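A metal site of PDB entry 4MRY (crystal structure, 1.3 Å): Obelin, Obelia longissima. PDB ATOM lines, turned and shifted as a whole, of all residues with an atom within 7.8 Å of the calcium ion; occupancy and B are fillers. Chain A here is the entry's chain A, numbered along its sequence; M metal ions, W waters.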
ATOM      1  N   PHE A 119      20.129  -6.302  10.072  1.00  0.00           N
ATOM      2  CA  PHE A 119      19.353  -7.530  10.090  1.00  0.00           C
ATOM      3  C   PHE A 119      20.033  -8.594  10.959  1.00  0.00           C
ATOM      4  O   PHE A 119      19.369  -9.267  11.756  1.00  0.00           O
ATOM      5  CB  PHE A 119      19.185  -8.058   8.664  1.00  0.00           C
ATOM      6  CG  PHE A 119      18.219  -9.199   8.543  1.00  0.00           C
ATOM      7  CD1 PHE A 119      18.656 -10.512   8.693  1.00  0.00           C
ATOM      8  CD2 PHE A 119      16.876  -8.972   8.231  1.00  0.00           C
ATOM      9  CE1 PHE A 119      17.769 -11.577   8.553  1.00  0.00           C
ATOM     10  CE2 PHE A 119      15.990 -10.037   8.091  1.00  0.00           C
ATOM     11  CZ  PHE A 119      16.438 -11.338   8.258  1.00  0.00           C
ATOM     12  N   PHE A 122      19.371  -7.742  14.581  1.00  0.00           N
ATOM     13  CA  PHE A 122      17.998  -8.046  14.983  1.00  0.00           C
ATOM     14  C   PHE A 122      17.714  -9.544  15.043  1.00  0.00           C
ATOM     15  O   PHE A 122      16.899  -9.980  15.849  1.00  0.00           O
ATOM     16  CB  PHE A 122      16.995  -7.444  13.993  1.00  0.00           C
ATOM     17  CG  PHE A 122      16.886  -5.934  14.020  1.00  0.00           C
ATOM     18  CD1 PHE A 122      17.168  -5.204  15.164  1.00  0.00           C
ATOM     19  CD2 PHE A 122      16.465  -5.256  12.885  1.00  0.00           C
ATOM     20  CE1 PHE A 122      17.038  -3.819  15.160  1.00  0.00           C
ATOM     21  CE2 PHE A 122      16.327  -3.871  12.876  1.00  0.00           C
ATOM     22  CZ  PHE A 122      16.619  -3.164  14.006  1.00  0.00           C
ATOM     23  N   ASP A 123      18.378 -10.310  14.196  1.00  0.00           N
ATOM     24  CA  ASP A 123      18.162 -11.748  14.110  1.00  0.00           C
ATOM     25  C   ASP A 123      18.972 -12.509  15.153  1.00  0.00           C
ATOM     26  O   ASP A 123      20.034 -13.050  14.865  1.00  0.00           O
ATOM     27  CB  ASP A 123      18.536 -12.236  12.713  1.00  0.00           C
ATOM     28  CG  ASP A 123      18.307 -13.716  12.541  1.00  0.00           C
ATOM     29  OD1 ASP A 123      17.474 -14.285  13.258  1.00  0.00           O
ATOM     30  OD2 ASP A 123      18.993 -14.293  11.679  1.00  0.00           O
ATOM     31  N   LYS A 124      18.552 -12.274  16.388  1.00  0.00           N
ATOM     32  CA  LYS A 124      19.347 -12.676  17.549  1.00  0.00           C
ATOM     33  C   LYS A 124      19.651 -14.172  17.589  1.00  0.00           C
ATOM     34  O   LYS A 124      20.645 -14.593  18.194  1.00  0.00           O
ATOM     35  CB  LYS A 124      18.670 -12.214  18.845  1.00  0.00           C
ATOM     36  CG  LYS A 124      18.744 -10.698  19.102  1.00  0.00           C
ATOM     37  CD  LYS A 124      20.147 -10.254  19.462  1.00  0.00           C
ATOM     38  CE  LYS A 124      20.212  -8.754  19.753  1.00  0.00           C
ATOM     39  NZ  LYS A 124      21.564  -8.353  20.231  1.00  0.00           N
ATOM     40  N   ASP A 125      17.381 -15.112  17.500  1.00  0.00           N
ATOM     41  CA  ASP A 125      17.304 -16.545  17.713  1.00  0.00           C
ATOM     42  C   ASP A 125      18.086 -17.238  16.606  1.00  0.00           C
ATOM     43  O   ASP A 125      18.056 -18.458  16.455  1.00  0.00           O
ATOM     44  CB  ASP A 125      15.860 -17.034  17.767  1.00  0.00           C
ATOM     45  CG  ASP A 125      15.095 -16.748  16.499  1.00  0.00           C
ATOM     46  OD1 ASP A 125      15.709 -16.460  15.448  1.00  0.00           O
ATOM     47  OD2 ASP A 125      13.852 -16.829  16.555  1.00  0.00           O
ATOM     48  N   GLY A 126      18.839 -16.463  15.829  1.00  0.00           N
ATOM     49  CA  GLY A 126      19.717 -16.996  14.799  1.00  0.00           C
ATOM     50  C   GLY A 126      19.088 -17.844  13.683  1.00  0.00           C
ATOM     51  O   GLY A 126      19.502 -18.966  13.449  1.00  0.00           O
ATOM     52  N   SER A 127      18.361 -17.195  12.797  1.00  0.00           N
ATOM     53  CA  SER A 127      17.425 -18.020  12.018  1.00  0.00           C
ATOM     54  C   SER A 127      17.402 -17.588  10.557  1.00  0.00           C
ATOM     55  O   SER A 127      16.877 -18.312   9.709  1.00  0.00           O
ATOM     56  CB  SER A 127      16.013 -17.937  12.590  1.00  0.00           C
ATOM     57  OG  SER A 127      15.403 -16.691  12.274  1.00  0.00           O
ATOM     58  N   GLY A 128      17.936 -16.409  10.275  1.00  0.00           N
ATOM     59  CA  GLY A 128      17.902 -15.847   8.944  1.00  0.00           C
ATOM     60  C   GLY A 128      16.609 -15.107   8.637  1.00  0.00           C
ATOM     61  O   GLY A 128      16.413 -14.643   7.527  1.00  0.00           O
ATOM     62  N   THR A 129      15.731 -15.002   9.634  1.00  0.00           N
ATOM     63  CA  THR A 129      14.448 -14.329   9.428  1.00  0.00           C
ATOM     64  C   THR A 129      14.200 -13.476  10.636  1.00  0.00           C
ATOM     65  O   THR A 129      14.686 -13.795  11.675  1.00  0.00           O
ATOM     66  CB  THR A 129      13.299 -15.340   9.335  1.00  0.00           C
ATOM     67  OG1 THR A 129      13.290 -16.142  10.515  1.00  0.00           O
ATOM     68  CG2 THR A 129      13.477 -16.234   8.109  1.00  0.00           C
ATOM     69  N   ILE A 130      13.441 -12.400  10.525  1.00  0.00           N
ATOM     70  CA  ILE A 130      13.062 -11.666  11.725  1.00  0.00           C
ATOM     71  C   ILE A 130      11.590 -11.946  12.057  1.00  0.00           C
ATOM     72  O   ILE A 130      10.713 -11.731  11.221  1.00  0.00           O
ATOM     73  CB  ILE A 130      13.258 -10.137  11.577  1.00  0.00           C
ATOM     74  CG1 ILE A 130      14.732  -9.798  11.383  1.00  0.00           C
ATOM     75  CG2 ILE A 130      12.708  -9.387  12.782  1.00  0.00           C
ATOM     76  CD1 ILE A 130      14.960  -8.326  11.120  1.00  0.00           C
ATOM     77  N   THR A 131      11.326 -12.427  13.249  1.00  0.00           N
ATOM     78  CA  THR A 131       9.941 -12.645  13.607  1.00  0.00           C
ATOM     79  C   THR A 131       9.437 -11.513  14.505  1.00  0.00           C
ATOM     80  O   THR A 131      10.204 -10.644  14.898  1.00  0.00           O
ATOM     81  CB  THR A 131       9.732 -14.059  14.164  1.00  0.00           C
ATOM     82  OG1 THR A 131      10.844 -14.404  14.983  1.00  0.00           O
ATOM     83  CG2 THR A 131       9.659 -15.067  13.019  1.00  0.00           C
ATOM     84  N   ASP A 133       8.545 -11.264  17.495  1.00  0.00           N
ATOM     85  CA  ASP A 133       9.204 -11.182  18.782  1.00  0.00           C
ATOM     86  C   ASP A 133      10.488 -10.349  18.702  1.00  0.00           C
ATOM     87  O   ASP A 133      10.734  -9.480  19.523  1.00  0.00           O
ATOM     88  CB  ASP A 133       9.450 -12.583  19.375  1.00  0.00           C
ATOM     89  CG  ASP A 133      10.062 -13.610  18.375  1.00  0.00           C
ATOM     90  OD1 ASP A 133      10.453 -13.257  17.238  1.00  0.00           O
ATOM     91  OD2 ASP A 133      10.150 -14.791  18.769  1.00  0.00           O
ATOM     92  N   GLU A 134      11.276 -10.615  17.693  1.00  0.00           N
ATOM     93  CA  GLU A 134      12.554  -9.921  17.472  1.00  0.00           C
ATOM     94  C   GLU A 134      12.414  -8.501  16.971  1.00  0.00           C
ATOM     95  O   GLU A 134      13.265  -7.640  17.239  1.00  0.00           O
ATOM     96  CB  GLU A 134      13.404 -10.692  16.471  1.00  0.00           C
ATOM     97  CG  GLU A 134      13.911 -11.988  17.004  1.00  0.00           C
ATOM     98  CD  GLU A 134      14.467 -12.822  15.926  1.00  0.00           C
ATOM     99  OE1 GLU A 134      13.927 -12.756  14.792  1.00  0.00           O
ATOM    100  OE2 GLU A 134      15.466 -13.558  16.206  1.00  0.00           O
ATOM    101  N   ASP A 165       7.271 -13.547   9.005  1.00  0.00           N
ATOM    102  CA  ASP A 165       8.661 -13.257   9.343  1.00  0.00           C
ATOM    103  C   ASP A 165       9.223 -12.331   8.294  1.00  0.00           C
ATOM    104  O   ASP A 165       8.658 -12.243   7.250  1.00  0.00           O
ATOM    105  CB  ASP A 165       9.497 -14.555   9.466  1.00  0.00           C
ATOM    106  CG  ASP A 165       9.428 -15.453   8.234  1.00  0.00           C
ATOM    107  OD1 ASP A 165       8.899 -15.064   7.181  1.00  0.00           O
ATOM    108  OD2 ASP A 165       9.927 -16.594   8.327  1.00  0.00           O
ATOM    109  N   LEU A 166      10.303 -11.599   8.553  1.00  0.00           N
ATOM    110  CA  LEU A 166      10.861 -10.710   7.532  1.00  0.00           C
ATOM    111  C   LEU A 166      12.178 -11.250   7.002  1.00  0.00           C
ATOM    112  O   LEU A 166      12.994 -11.762   7.793  1.00  0.00           O
ATOM    113  CB  LEU A 166      11.108  -9.299   8.102  1.00  0.00           C
ATOM    114  CG  LEU A 166      10.023  -8.719   8.987  1.00  0.00           C
ATOM    115  CD1 LEU A 166      10.450  -7.375   9.543  1.00  0.00           C
ATOM    116  CD2 LEU A 166       8.693  -8.593   8.227  1.00  0.00           C
HETATM  117 CA    CA M   1      15.271 -14.817  13.903  1.00  0.00          CA
HETATM  118  O   HOH W   1      13.082 -15.766  14.221  1.00  0.00           O
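OD2 of Asp 123 is in hydrogen-bond range of N of Gly 128 (2.8 Å). The backbone NH (N) of Thr 131 lies close to the side-chain carboxylate (OE1) of Glu 134. The side-chain carboxylate of Glu 134 lies close to the backbone NH of Lys 124, 3.3 Å away.
Of the 15 residues printed, 5 come within 4 Å of the calcium ion.
The calcium ion is bound by OD1 of Asp 125 (2.3 Å), OD1 of Asp 123 (2.4 Å), water W1 (2.4 Å), OG of Ser 127 (2.5 Å), O of Thr 129 (2.5 Å), OE1 of Glu 134 (2.6 Å) and OE2 of Glu 134 (2.6 Å).
Water W1 bridges the side-chain carboxylate (OD2) of Asp 125 (2.7 Å) and the side-chain hydroxyl (OG1) of Thr 131 (2.7 Å).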
